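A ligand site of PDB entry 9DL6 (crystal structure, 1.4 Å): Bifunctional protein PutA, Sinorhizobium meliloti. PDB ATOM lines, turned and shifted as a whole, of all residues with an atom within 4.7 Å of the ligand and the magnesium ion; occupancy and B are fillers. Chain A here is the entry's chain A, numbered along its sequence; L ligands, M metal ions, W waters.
The magnesium ion is bound by water W11 (2.0 Å), water W3 (2.0 Å), O2 of the ligand (2.0 Å), water W5 (2.1 Å), water W4 (2.2 Å) and water W7 (2.2 Å).
Water W11 lies within hydrogen-bond range of O8 of the ligand (2.7 Å) and OE2 of Glu 736 (2.9 Å). Water W4 bridges OE2 of Glu 735 and O3 of the ligand. Water W10 bridges O9 of the ligand and OE1 of Glu 736. Water W8 lies within hydrogen-bond range of O of Ser 1018 (2.7 Å), OE1 of Glu 812 (2.7 Å) and N7 of the ligand (3.1 Å). Water W1 lies within hydrogen-bond range of OE1 of Glu 942, O12 of the ligand and N of Gly 814.
An oxygen (O11) of the ligand lies close to the backbone carbonyl oxygen (O) of Gly 784 (3.3 Å). Merely in contact with the ligand: Ile 705 (3.2 Å), Pro 707 (3.1 Å), Asn 709 (3.3 Å), Phe 710 (3.9 Å), Ile 714 (3.3 Å), Pro 733 (3.7 Å), Asp 764 (3.7 Å), Gly 765 (3.5 Å), Gly 768 (3.4 Å), Ala 769 (3.4 Å), Phe 782 (3.3 Å), Thr 783 (3.3 Å), Val 788 (3.3 Å), Ile 792 (3.7 Å), Glu 812 (3.4 Å), Gly 814 (3.3 Å), Phe 944 (3.4 Å), Leu 972 (3.9 Å), Phe 1012 (3.2 Å) and Ser 1018 (3.9 Å). Hydrophobic or aromatic side chains that line the ligand: Ile 705, Pro 707, Trp 708, Phe 710, Ile 714, Ala 769, Phe 782, Val 788, Ile 792, Phe 944, Leu 972 and Phe 1012.
An oxygen (O1) of the ligand lies within hydrogen-bond range of the backbone NH (N) of Ser 785, at 2.9 Å. An oxygen (O1) of the ligand lies within hydrogen-bond range of the side-chain hydroxyl (OG) of Ser 785. The side-chain amino group of Lys 732 is in hydrogen-bond range of an oxygen (O6) of the ligand (2.6 Å). O12 of the ligand is in hydrogen-bond range of OE1 of Glu 942 (2.7 Å). OE1 of Glu 735 lies within hydrogen-bond range of O6 of the ligand (2.7 Å). The backbone carbonyl oxygen (O) of Thr 813 is in hydrogen-bond range of a nitrogen (N7) of the ligand (2.7 Å). O of Ser 706 sits at hydrogen-bond distance from O5 of the ligand (2.8 Å). O14 of the ligand lies close to SG of Cys 846 (3.7 Å). N of Trp 708 lies within hydrogen-bond range of O9 of the ligand (3.0 Å). The backbone NH (N) of Ala 734 lies close to an oxygen (O5) of the ligand (3.5 Å).
The backbone NH (N) of Val 788 sits close to the side-chain hydroxyl (OG) of Ser 785, at 3.3 Å. The side-chain amino group of Lys 732 lies within hydrogen-bond range of the backbone carbonyl oxygen of Gly 763, 2.7 Å away. The side-chain carboxylate (OE2) of Glu 942 sits at hydrogen-bond distance from the backbone NH (N) of Gly 815 (3.0 Å). O of Ser 706 sits at hydrogen-bond distance from N of Ala 734. The backbone carbonyl oxygen (O) of Ile 705 lies within hydrogen-bond range of the backbone NH (N) of Thr 783 (3.1 Å). The backbone carbonyl oxygen (O) of Phe 782 sits at hydrogen-bond distance from the backbone NH (N) of Glu 812 (2.9 Å). The side-chain hydroxyl of Ser 1018 lies within hydrogen-bond range of the backbone carbonyl oxygen of Gly 814. The side-chain hydroxyl (OG) of Ser 1018 sits at hydrogen-bond distance from the backbone NH (N) of Leu 972 (3.4 Å).
No residue comes within 4 Å of the magnesium ion.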
ATOM      1  N   ILE A 705     -19.911  29.376  22.600  1.00  0.00           N
ATOM      2  CA  ILE A 705     -19.593  28.467  23.682  1.00  0.00           C
ATOM      3  C   ILE A 705     -18.210  27.907  23.368  1.00  0.00           C
ATOM      4  O   ILE A 705     -18.000  27.348  22.286  1.00  0.00           O
ATOM      5  CB  ILE A 705     -20.652  27.365  23.779  1.00  0.00           C
ATOM      6  CG1 ILE A 705     -21.977  27.968  24.225  1.00  0.00           C
ATOM      7  CG2 ILE A 705     -20.234  26.287  24.751  1.00  0.00           C
ATOM      8  CD1 ILE A 705     -23.167  27.059  23.958  1.00  0.00           C
ATOM      9  N   SER A 706     -17.272  28.088  24.296  1.00  0.00           N
ATOM     10  CA  SER A 706     -15.875  27.774  24.038  1.00  0.00           C
ATOM     11  C   SER A 706     -15.344  26.776  25.051  1.00  0.00           C
ATOM     12  O   SER A 706     -15.903  26.606  26.141  1.00  0.00           O
ATOM     13  CB  SER A 706     -15.028  29.049  24.040  1.00  0.00           C
ATOM     14  OG  SER A 706     -15.288  29.813  25.191  1.00  0.00           O
ATOM     15  N   PRO A 707     -14.255  26.092  24.720  1.00  0.00           N
ATOM     16  CA  PRO A 707     -13.700  25.074  25.612  1.00  0.00           C
ATOM     17  C   PRO A 707     -12.644  25.673  26.532  1.00  0.00           C
ATOM     18  O   PRO A 707     -12.200  26.809  26.360  1.00  0.00           O
ATOM     19  CB  PRO A 707     -13.045  24.109  24.625  1.00  0.00           C
ATOM     20  CG  PRO A 707     -12.545  24.999  23.574  1.00  0.00           C
ATOM     21  CD  PRO A 707     -13.588  26.084  23.410  1.00  0.00           C
ATOM     22  N   TRP A 708     -12.236  24.881  27.517  1.00  0.00           N
ATOM     23  CA  TRP A 708     -11.275  25.408  28.481  1.00  0.00           C
ATOM     24  C   TRP A 708      -9.853  25.420  27.933  1.00  0.00           C
ATOM     25  O   TRP A 708      -9.013  26.167  28.448  1.00  0.00           O
ATOM     26  CB  TRP A 708     -11.304  24.603  29.791  1.00  0.00           C
ATOM     27  CG  TRP A 708     -10.685  23.274  29.588  1.00  0.00           C
ATOM     28  CD1 TRP A 708     -11.319  22.125  29.300  1.00  0.00           C
ATOM     29  CD2 TRP A 708      -9.271  22.978  29.610  1.00  0.00           C
ATOM     30  NE1 TRP A 708     -10.406  21.111  29.138  1.00  0.00           N
ATOM     31  CE2 TRP A 708      -9.149  21.613  29.315  1.00  0.00           C
ATOM     32  CE3 TRP A 708      -8.110  23.728  29.845  1.00  0.00           C
ATOM     33  CZ2 TRP A 708      -7.912  20.975  29.253  1.00  0.00           C
ATOM     34  CZ3 TRP A 708      -6.885  23.095  29.778  1.00  0.00           C
ATOM     35  CH2 TRP A 708      -6.791  21.731  29.495  1.00  0.00           C
ATOM     36  N   ASN A 709      -9.571  24.608  26.910  1.00  0.00           N
ATOM     37  CA  ASN A 709      -8.190  24.296  26.576  1.00  0.00           C
ATOM     38  C   ASN A 709      -7.529  25.330  25.693  1.00  0.00           C
ATOM     39  O   ASN A 709      -6.299  25.353  25.593  1.00  0.00           O
ATOM     40  CB  ASN A 709      -8.097  22.900  25.960  1.00  0.00           C
ATOM     41  CG  ASN A 709      -8.759  22.821  24.603  1.00  0.00           C
ATOM     42  OD1 ASN A 709      -9.828  23.368  24.379  1.00  0.00           O
ATOM     43  ND2 ASN A 709      -8.119  22.115  23.679  1.00  0.00           N
ATOM     44  N   PHE A 710      -8.306  26.185  25.044  1.00  0.00           N
ATOM     45  CA  PHE A 710      -7.791  27.377  24.384  1.00  0.00           C
ATOM     46  C   PHE A 710      -8.641  28.526  24.879  1.00  0.00           C
ATOM     47  O   PHE A 710      -9.444  29.109  24.136  1.00  0.00           O
ATOM     48  CB  PHE A 710      -7.796  27.233  22.863  1.00  0.00           C
ATOM     49  CG  PHE A 710      -6.860  26.161  22.391  1.00  0.00           C
ATOM     50  CD1 PHE A 710      -5.506  26.432  22.252  1.00  0.00           C
ATOM     51  CD2 PHE A 710      -7.323  24.893  22.138  1.00  0.00           C
ATOM     52  CE1 PHE A 710      -4.637  25.449  21.841  1.00  0.00           C
ATOM     53  CE2 PHE A 710      -6.437  23.899  21.717  1.00  0.00           C
ATOM     54  CZ  PHE A 710      -5.096  24.186  21.580  1.00  0.00           C
ATOM     55  N   ILE A 714      -9.551  30.386  21.203  1.00  0.00           N
ATOM     56  CA  ILE A 714     -10.806  29.964  20.595  1.00  0.00           C
ATOM     57  C   ILE A 714     -11.948  30.830  21.087  1.00  0.00           C
ATOM     58  O   ILE A 714     -12.851  31.197  20.325  1.00  0.00           O
ATOM     59  CB  ILE A 714     -11.063  28.467  20.849  1.00  0.00           C
ATOM     60  CG1 ILE A 714     -10.046  27.646  20.043  1.00  0.00           C
ATOM     61  CG2 ILE A 714     -12.511  28.096  20.499  1.00  0.00           C
ATOM     62  CD1 ILE A 714     -10.163  26.176  20.264  1.00  0.00           C
ATOM     63  N   LYS A 732     -20.149  32.414  26.378  1.00  0.00           N
ATOM     64  CA  LYS A 732     -20.239  31.473  27.490  1.00  0.00           C
ATOM     65  C   LYS A 732     -18.920  30.711  27.527  1.00  0.00           C
ATOM     66  O   LYS A 732     -18.757  29.695  26.834  1.00  0.00           O
ATOM     67  CB  LYS A 732     -21.419  30.539  27.320  1.00  0.00           C
ATOM     68  CG  LYS A 732     -22.071  30.098  28.615  1.00  0.00           C
ATOM     69  CD  LYS A 732     -21.098  29.354  29.525  1.00  0.00           C
ATOM     70  CE  LYS A 732     -20.717  28.010  28.941  1.00  0.00           C
ATOM     71  NZ  LYS A 732     -19.774  27.328  29.876  1.00  0.00           N
ATOM     72  N   PRO A 733     -17.941  31.164  28.302  1.00  0.00           N
ATOM     73  CA  PRO A 733     -16.676  30.451  28.394  1.00  0.00           C
ATOM     74  C   PRO A 733     -16.811  29.187  29.218  1.00  0.00           C
ATOM     75  O   PRO A 733     -17.723  29.031  30.026  1.00  0.00           O
ATOM     76  CB  PRO A 733     -15.765  31.445  29.107  1.00  0.00           C
ATOM     77  CG  PRO A 733     -16.695  32.232  29.968  1.00  0.00           C
ATOM     78  CD  PRO A 733     -17.969  32.366  29.163  1.00  0.00           C
ATOM     79  N   ALA A 734     -15.866  28.275  28.996  1.00  0.00           N
ATOM     80  CA  ALA A 734     -15.823  27.045  29.775  1.00  0.00           C
ATOM     81  C   ALA A 734     -15.777  27.384  31.264  1.00  0.00           C
ATOM     82  O   ALA A 734     -15.136  28.357  31.679  1.00  0.00           O
ATOM     83  CB  ALA A 734     -14.566  26.265  29.424  1.00  0.00           C
ATOM     84  N   GLU A 735     -16.459  26.559  32.062  1.00  0.00           N
ATOM     85  CA  GLU A 735     -16.499  26.805  33.491  1.00  0.00           C
ATOM     86  C   GLU A 735     -15.109  26.759  34.129  1.00  0.00           C
ATOM     87  O   GLU A 735     -14.907  27.391  35.183  1.00  0.00           O
ATOM     88  CB  GLU A 735     -17.418  25.802  34.187  1.00  0.00           C
ATOM     89  CG  GLU A 735     -17.086  24.338  33.923  1.00  0.00           C
ATOM     90  CD  GLU A 735     -17.824  23.779  32.720  1.00  0.00           C
ATOM     91  OE1 GLU A 735     -18.157  24.553  31.794  1.00  0.00           O
ATOM     92  OE2 GLU A 735     -18.080  22.548  32.697  1.00  0.00           O
ATOM     93  N   GLU A 736     -14.157  26.062  33.531  1.00  0.00           N
ATOM     94  CA  GLU A 736     -12.841  25.935  34.150  1.00  0.00           C
ATOM     95  C   GLU A 736     -12.010  27.204  34.003  1.00  0.00           C
ATOM     96  O   GLU A 736     -11.140  27.470  34.827  1.00  0.00           O
ATOM     97  CB  GLU A 736     -12.080  24.752  33.551  1.00  0.00           C
ATOM     98  CG  GLU A 736     -12.773  23.405  33.728  1.00  0.00           C
ATOM     99  CD  GLU A 736     -13.660  23.022  32.543  1.00  0.00           C
ATOM    100  OE1 GLU A 736     -14.099  23.921  31.788  1.00  0.00           O
ATOM    101  OE2 GLU A 736     -13.916  21.810  32.371  1.00  0.00           O
ATOM    102  N   GLY A 763     -20.238  30.369  33.588  1.00  0.00           N
ATOM    103  CA  GLY A 763     -21.020  29.295  34.155  1.00  0.00           C
ATOM    104  C   GLY A 763     -20.724  27.989  33.437  1.00  0.00           C
ATOM    105  O   GLY A 763     -19.887  27.924  32.541  1.00  0.00           O
ATOM    106  N   ASP A 764     -21.456  26.962  33.850  1.00  0.00           N
ATOM    107  CA  ASP A 764     -21.215  25.620  33.345  1.00  0.00           C
ATOM    108  C   ASP A 764     -22.097  25.352  32.120  1.00  0.00           C
ATOM    109  O   ASP A 764     -22.635  26.285  31.505  1.00  0.00           O
ATOM    110  CB  ASP A 764     -21.378  24.591  34.475  1.00  0.00           C
ATOM    111  CG  ASP A 764     -22.762  24.619  35.100  1.00  0.00           C
ATOM    112  OD1 ASP A 764     -23.761  24.610  34.347  1.00  0.00           O
ATOM    113  OD2 ASP A 764     -22.866  24.633  36.345  1.00  0.00           O
ATOM    114  N   GLY A 765     -22.256  24.079  31.747  1.00  0.00           N
ATOM    115  CA  GLY A 765     -23.049  23.740  30.581  1.00  0.00           C
ATOM    116  C   GLY A 765     -24.496  24.178  30.678  1.00  0.00           C
ATOM    117  O   GLY A 765     -25.135  24.372  29.645  1.00  0.00           O
ATOM    118  N   GLY A 768     -24.683  27.454  29.039  1.00  0.00           N
ATOM    119  CA  GLY A 768     -24.619  27.255  27.603  1.00  0.00           C
ATOM    120  C   GLY A 768     -25.931  26.739  27.046  1.00  0.00           C
ATOM    121  O   GLY A 768     -26.418  27.219  26.016  1.00  0.00           O
ATOM    122  N   ALA A 769     -26.538  25.765  27.732  1.00  0.00           N
ATOM    123  CA  ALA A 769     -27.794  25.187  27.247  1.00  0.00           C
ATOM    124  C   ALA A 769     -28.913  26.206  27.290  1.00  0.00           C
ATOM    125  O   ALA A 769     -29.733  26.274  26.359  1.00  0.00           O
ATOM    126  CB  ALA A 769     -28.154  23.953  28.066  1.00  0.00           C
ATOM    127  N   VAL A 772     -28.418  28.427  24.336  1.00  0.00           N
ATOM    128  CA  VAL A 772     -28.765  27.743  23.105  1.00  0.00           C
ATOM    129  C   VAL A 772     -30.274  27.689  22.923  1.00  0.00           C
ATOM    130  O   VAL A 772     -30.791  27.905  21.815  1.00  0.00           O
ATOM    131  CB  VAL A 772     -28.134  26.337  23.073  1.00  0.00           C
ATOM    132  CG1 VAL A 772     -28.721  25.508  21.938  1.00  0.00           C
ATOM    133  CG2 VAL A 772     -26.618  26.448  22.894  1.00  0.00           C
ATOM    134  N   PHE A 782     -19.927  26.653  18.588  1.00  0.00           N
ATOM    135  CA  PHE A 782     -19.519  25.755  19.650  1.00  0.00           C
ATOM    136  C   PHE A 782     -18.175  25.148  19.295  1.00  0.00           C
ATOM    137  O   PHE A 782     -17.985  24.656  18.179  1.00  0.00           O
ATOM    138  CB  PHE A 782     -20.530  24.622  19.823  1.00  0.00           C
ATOM    139  CG  PHE A 782     -20.089  23.585  20.810  1.00  0.00           C
ATOM    140  CD1 PHE A 782     -20.231  23.817  22.167  1.00  0.00           C
ATOM    141  CD2 PHE A 782     -19.523  22.403  20.392  1.00  0.00           C
ATOM    142  CE1 PHE A 782     -19.829  22.878  23.090  1.00  0.00           C
ATOM    143  CE2 PHE A 782     -19.115  21.457  21.313  1.00  0.00           C
ATOM    144  CZ  PHE A 782     -19.272  21.693  22.651  1.00  0.00           C
ATOM    145  N   THR A 783     -17.264  25.173  20.249  1.00  0.00           N
ATOM    146  CA  THR A 783     -16.046  24.391  20.184  1.00  0.00           C
ATOM    147  C   THR A 783     -15.950  23.621  21.485  1.00  0.00           C
ATOM    148  O   THR A 783     -16.062  24.193  22.568  1.00  0.00           O
ATOM    149  CB  THR A 783     -14.829  25.273  19.949  1.00  0.00           C
ATOM    150  OG1 THR A 783     -15.022  26.001  18.724  1.00  0.00           O
ATOM    151  CG2 THR A 783     -13.587  24.427  19.788  1.00  0.00           C
ATOM    152  N   GLY A 784     -15.805  22.301  21.370  1.00  0.00           N
ATOM    153  CA  GLY A 784     -15.874  21.453  22.546  1.00  0.00           C
ATOM    154  C   GLY A 784     -16.003  20.004  22.138  1.00  0.00           C
ATOM    155  O   GLY A 784     -15.671  19.639  21.019  1.00  0.00           O
ATOM    156  N   SER A 785     -16.486  19.193  23.065  1.00  0.00           N
ATOM    157  CA  SER A 785     -16.578  17.757  22.796  1.00  0.00           C
ATOM    158  C   SER A 785     -17.702  17.452  21.820  1.00  0.00           C
ATOM    159  O   SER A 785     -18.709  18.161  21.731  1.00  0.00           O
ATOM    160  CB  SER A 785     -16.804  17.003  24.105  1.00  0.00           C
ATOM    161  OG  SER A 785     -18.040  17.375  24.688  1.00  0.00           O
ATOM    162  N   VAL A 788     -21.117  16.896  23.601  1.00  0.00           N
ATOM    163  CA  VAL A 788     -21.865  18.106  23.941  1.00  0.00           C
ATOM    164  C   VAL A 788     -22.426  18.757  22.687  1.00  0.00           C
ATOM    165  O   VAL A 788     -23.574  19.221  22.683  1.00  0.00           O
ATOM    166  CB  VAL A 788     -21.004  19.061  24.773  1.00  0.00           C
ATOM    167  CG1 VAL A 788     -21.694  20.414  24.896  1.00  0.00           C
ATOM    168  CG2 VAL A 788     -20.756  18.472  26.154  1.00  0.00           C
ATOM    169  N   LEU A 791     -25.671  17.217  21.894  1.00  0.00           N
ATOM    170  CA  LEU A 791     -26.776  17.709  22.705  1.00  0.00           C
ATOM    171  C   LEU A 791     -27.238  19.067  22.197  1.00  0.00           C
ATOM    172  O   LEU A 791     -28.440  19.333  22.133  1.00  0.00           O
ATOM    173  CB  LEU A 791     -26.340  17.808  24.156  1.00  0.00           C
ATOM    174  CG  LEU A 791     -26.107  16.472  24.867  1.00  0.00           C
ATOM    175  CD1 LEU A 791     -25.462  16.707  26.211  1.00  0.00           C
ATOM    176  CD2 LEU A 791     -27.421  15.724  25.028  1.00  0.00           C
ATOM    177  N   ILE A 792     -26.290  19.944  21.837  1.00  0.00           N
ATOM    178  CA  ILE A 792     -26.670  21.227  21.259  1.00  0.00           C
ATOM    179  C   ILE A 792     -27.418  21.032  19.948  1.00  0.00           C
ATOM    180  O   ILE A 792     -28.429  21.696  19.690  1.00  0.00           O
ATOM    181  CB  ILE A 792     -25.428  22.122  21.115  1.00  0.00           C
ATOM    182  CG1 ILE A 792     -24.942  22.547  22.494  1.00  0.00           C
ATOM    183  CG2 ILE A 792     -25.712  23.320  20.198  1.00  0.00           C
ATOM    184  CD1 ILE A 792     -23.563  23.160  22.482  1.00  0.00           C
ATOM    185  N   GLU A 812     -17.208  22.593  16.311  1.00  0.00           N
ATOM    186  CA  GLU A 812     -15.838  22.159  16.090  1.00  0.00           C
ATOM    187  C   GLU A 812     -15.473  21.292  17.269  1.00  0.00           C
ATOM    188  O   GLU A 812     -15.468  21.761  18.417  1.00  0.00           O
ATOM    189  CB  GLU A 812     -14.943  23.380  15.921  1.00  0.00           C
ATOM    190  CG  GLU A 812     -15.364  24.223  14.705  1.00  0.00           C
ATOM    191  CD  GLU A 812     -15.381  23.416  13.398  1.00  0.00           C
ATOM    192  OE1 GLU A 812     -14.301  23.204  12.818  1.00  0.00           O
ATOM    193  OE2 GLU A 812     -16.472  22.986  12.952  1.00  0.00           O
ATOM    194  N   THR A 813     -15.235  20.012  17.007  1.00  0.00           N
ATOM    195  CA  THR A 813     -15.242  19.007  18.058  1.00  0.00           C
ATOM    196  C   THR A 813     -13.955  18.205  18.103  1.00  0.00           C
ATOM    197  O   THR A 813     -12.902  18.686  17.684  1.00  0.00           O
ATOM    198  CB  THR A 813     -16.507  18.149  17.944  1.00  0.00           C
ATOM    199  OG1 THR A 813     -16.672  17.689  16.583  1.00  0.00           O
ATOM    200  CG2 THR A 813     -17.731  18.992  18.302  1.00  0.00           C
ATOM    201  N   GLY A 814     -14.025  16.979  18.626  1.00  0.00           N
ATOM    202  CA  GLY A 814     -12.824  16.259  19.000  1.00  0.00           C
ATOM    203  C   GLY A 814     -12.078  15.648  17.839  1.00  0.00           C
ATOM    204  O   GLY A 814     -12.498  15.705  16.680  1.00  0.00           O
ATOM    205  N   GLY A 815     -10.943  15.029  18.161  1.00  0.00           N
ATOM    206  CA  GLY A 815     -10.141  14.364  17.158  1.00  0.00           C
ATOM    207  C   GLY A 815      -9.613  13.052  17.696  1.00  0.00           C
ATOM    208  O   GLY A 815      -9.607  12.813  18.901  1.00  0.00           O
ATOM    209  N   CYS A 846      -7.049  19.848  21.008  1.00  0.00           N
ATOM    210  CA  CYS A 846      -7.871  19.022  20.139  1.00  0.00           C
ATOM    211  C   CYS A 846      -7.057  18.419  19.010  1.00  0.00           C
ATOM    212  O   CYS A 846      -7.388  17.347  18.510  1.00  0.00           O
ATOM    213  CB  CYS A 846      -9.020  19.861  19.580  1.00  0.00           C
ATOM    214  SG  CYS A 846      -8.493  21.407  18.887  1.00  0.00           S
ATOM    215  N   GLU A 942     -11.912   9.552  22.088  1.00  0.00           N
ATOM    216  CA  GLU A 942     -10.890  10.574  22.291  1.00  0.00           C
ATOM    217  C   GLU A 942     -10.542  10.626  23.765  1.00  0.00           C
ATOM    218  O   GLU A 942     -11.434  10.812  24.616  1.00  0.00           O
ATOM    219  CB  GLU A 942     -11.399  11.938  21.826  1.00  0.00           C
ATOM    220  CG  GLU A 942     -10.419  13.096  22.083  1.00  0.00           C
ATOM    221  CD  GLU A 942     -11.052  14.471  21.890  1.00  0.00           C
ATOM    222  OE1 GLU A 942     -12.140  14.704  22.467  1.00  0.00           O
ATOM    223  OE2 GLU A 942     -10.466  15.297  21.158  1.00  0.00           O
ATOM    224  N   PHE A 944      -8.584  12.754  26.245  1.00  0.00           N
ATOM    225  CA  PHE A 944      -8.112  14.132  26.134  1.00  0.00           C
ATOM    226  C   PHE A 944      -7.068  14.389  27.219  1.00  0.00           C
ATOM    227  O   PHE A 944      -7.290  15.089  28.201  1.00  0.00           O
ATOM    228  CB  PHE A 944      -9.283  15.098  26.230  1.00  0.00           C
ATOM    229  CG  PHE A 944      -9.011  16.426  25.614  1.00  0.00           C
ATOM    230  CD1 PHE A 944      -8.894  16.541  24.234  1.00  0.00           C
ATOM    231  CD2 PHE A 944      -8.883  17.563  26.388  1.00  0.00           C
ATOM    232  CE1 PHE A 944      -8.610  17.779  23.658  1.00  0.00           C
ATOM    233  CE2 PHE A 944      -8.631  18.806  25.795  1.00  0.00           C
ATOM    234  CZ  PHE A 944      -8.485  18.898  24.445  1.00  0.00           C
ATOM    235  N   LEU A 972      -9.658  15.344  12.224  1.00  0.00           N
ATOM    236  CA  LEU A 972      -9.201  16.667  12.620  1.00  0.00           C
ATOM    237  C   LEU A 972      -7.782  16.900  12.115  1.00  0.00           C
ATOM    238  O   LEU A 972      -7.599  17.410  11.006  1.00  0.00           O
ATOM    239  CB  LEU A 972      -9.346  16.862  14.140  1.00  0.00           C
ATOM    240  CG  LEU A 972      -9.100  18.278  14.649  1.00  0.00           C
ATOM    241  CD1 LEU A 972      -9.950  19.287  13.859  1.00  0.00           C
ATOM    242  CD2 LEU A 972      -9.438  18.356  16.123  1.00  0.00           C
ATOM    243  N   PHE A1012      -8.072  26.037  10.470  1.00  0.00           N
ATOM    244  CA  PHE A1012      -8.126  24.880  11.334  1.00  0.00           C
ATOM    245  C   PHE A1012      -9.549  24.365  11.455  1.00  0.00           C
ATOM    246  O   PHE A1012     -10.465  25.133  11.731  1.00  0.00           O
ATOM    247  CB  PHE A1012      -7.600  25.190  12.740  1.00  0.00           C
ATOM    248  CG  PHE A1012      -7.543  23.976  13.618  1.00  0.00           C
ATOM    249  CD1 PHE A1012      -6.530  23.042  13.449  1.00  0.00           C
ATOM    250  CD2 PHE A1012      -8.508  23.745  14.586  1.00  0.00           C
ATOM    251  CE1 PHE A1012      -6.479  21.906  14.242  1.00  0.00           C
ATOM    252  CE2 PHE A1012      -8.463  22.616  15.380  1.00  0.00           C
ATOM    253  CZ  PHE A1012      -7.440  21.691  15.210  1.00  0.00           C
ATOM    254  N   SER A1018     -15.285  15.381  13.939  1.00  0.00           N
ATOM    255  CA  SER A1018     -14.422  16.463  14.358  1.00  0.00           C
ATOM    256  C   SER A1018     -14.973  17.846  14.017  1.00  0.00           C
ATOM    257  O   SER A1018     -14.403  18.844  14.473  1.00  0.00           O
ATOM    258  CB  SER A1018     -13.043  16.324  13.696  1.00  0.00           C
ATOM    259  OG  SER A1018     -12.450  15.123  14.134  1.00  0.00           O
HETATM  260  P1  LIG L   1     -16.814  20.436  26.627  1.00  0.00           P
HETATM  261  O1  LIG L   1     -17.700  19.712  25.655  1.00  0.00           O
HETATM  262  O2  LIG L   1     -16.748  19.717  27.944  1.00  0.00           O
HETATM  263  O3  LIG L   1     -17.313  21.978  26.938  1.00  0.00           O
HETATM  264  C1  LIG L   1     -17.095  23.036  25.996  1.00  0.00           C
HETATM  265  C2  LIG L   1     -18.130  24.153  26.373  1.00  0.00           C
HETATM  266  O4  LIG L   1     -19.608  23.538  26.270  1.00  0.00           O
HETATM  267  C3  LIG L   1     -18.002  24.601  27.594  1.00  0.00           C
HETATM  268  O5  LIG L   1     -18.174  26.091  27.606  1.00  0.00           O
HETATM  269  C4  LIG L   1     -19.166  23.959  28.417  1.00  0.00           C
HETATM  270  O6  LIG L   1     -19.509  24.738  29.490  1.00  0.00           O
HETATM  271  C5  LIG L   1     -20.274  23.887  27.381  1.00  0.00           C
HETATM  272  N1  LIG L   1     -21.216  22.829  27.702  1.00  0.00           N
HETATM  273  C6  LIG L   1     -21.177  21.673  28.365  1.00  0.00           C
HETATM  274  N2  LIG L   1     -22.403  21.117  28.251  1.00  0.00           N
HETATM  275  C7  LIG L   1     -23.179  21.951  27.520  1.00  0.00           C
HETATM  276  C8  LIG L   1     -24.518  21.845  27.120  1.00  0.00           C
HETATM  277  N3  LIG L   1     -25.330  20.667  27.517  1.00  0.00           N
HETATM  278  N4  LIG L   1     -25.055  22.801  26.399  1.00  0.00           N
HETATM  279  C9  LIG L   1     -24.306  23.900  26.019  1.00  0.00           C
HETATM  280  N5  LIG L   1     -23.010  24.013  26.412  1.00  0.00           N
HETATM  281  C10 LIG L   1     -22.453  23.013  27.169  1.00  0.00           C
HETATM  282  O7  LIG L   1     -15.311  20.577  26.014  1.00  0.00           O
HETATM  283  P2  LIG L   1     -13.950  21.146  26.812  1.00  0.00           P
HETATM  284  O8  LIG L   1     -13.599  20.131  27.908  1.00  0.00           O
HETATM  285  O9  LIG L   1     -14.085  22.540  27.349  1.00  0.00           O
HETATM  286  O10 LIG L   1     -12.793  21.041  25.648  1.00  0.00           O
HETATM  287  C11 LIG L   1     -12.360  19.726  25.303  1.00  0.00           C
HETATM  288  C12 LIG L   1     -12.974  19.165  24.024  1.00  0.00           C
HETATM  289  O11 LIG L   1     -13.036  20.341  22.942  1.00  0.00           O
HETATM  290  C13 LIG L   1     -12.233  18.202  23.470  1.00  0.00           C
HETATM  291  O12 LIG L   1     -13.168  17.129  22.919  1.00  0.00           O
HETATM  292  C14 LIG L   1     -11.501  18.841  22.332  1.00  0.00           C
HETATM  293  O13 LIG L   1     -11.138  17.951  21.303  1.00  0.00           O
HETATM  294  C15 LIG L   1     -12.591  19.840  21.851  1.00  0.00           C
HETATM  295  N6  LIG L   1     -11.918  20.918  21.099  1.00  0.00           N
HETATM  296  C16 LIG L   1     -12.103  21.013  19.728  1.00  0.00           C
HETATM  297  C17 LIG L   1     -11.439  22.034  19.095  1.00  0.00           C
HETATM  298  C18 LIG L   1     -11.567  22.233  17.560  1.00  0.00           C
HETATM  299  O14 LIG L   1     -11.155  23.231  17.071  1.00  0.00           O
HETATM  300  N7  LIG L   1     -12.152  21.142  16.759  1.00  0.00           N
HETATM  301  C19 LIG L   1     -10.669  22.943  19.800  1.00  0.00           C
HETATM  302  C20 LIG L   1     -10.473  22.810  21.152  1.00  0.00           C
HETATM  303  C21 LIG L   1     -11.129  21.769  21.789  1.00  0.00           C
HETATM  304 MG    MG M   1     -16.776  19.672  29.992  1.00  0.00          MG
HETATM  305  O   HOH W   1     -14.959  14.872  21.234  1.00  0.00           O
HETATM  306  O   HOH W   2     -14.631  17.531  27.375  1.00  0.00           O
HETATM  307  O   HOH W   3     -16.313  17.766  29.437  1.00  0.00           O
HETATM  308  O   HOH W   4     -17.582  21.659  30.168  1.00  0.00           O
HETATM  309  O   HOH W   5     -16.833  19.314  32.065  1.00  0.00           O
HETATM  310  O   HOH W   6     -11.518  25.440  15.785  1.00  0.00           O
HETATM  311  O   HOH W   7     -18.954  19.205  29.694  1.00  0.00           O
HETATM  312  O   HOH W   8     -13.010  21.024  13.827  1.00  0.00           O
HETATM  313  O   HOH W   9     -27.540  22.063  25.083  1.00  0.00           O
HETATM  314  O   HOH W  10     -15.572  23.137  29.586  1.00  0.00           O
HETATM  315  O   HOH W  11     -14.891  20.148  30.256  1.00  0.00           O
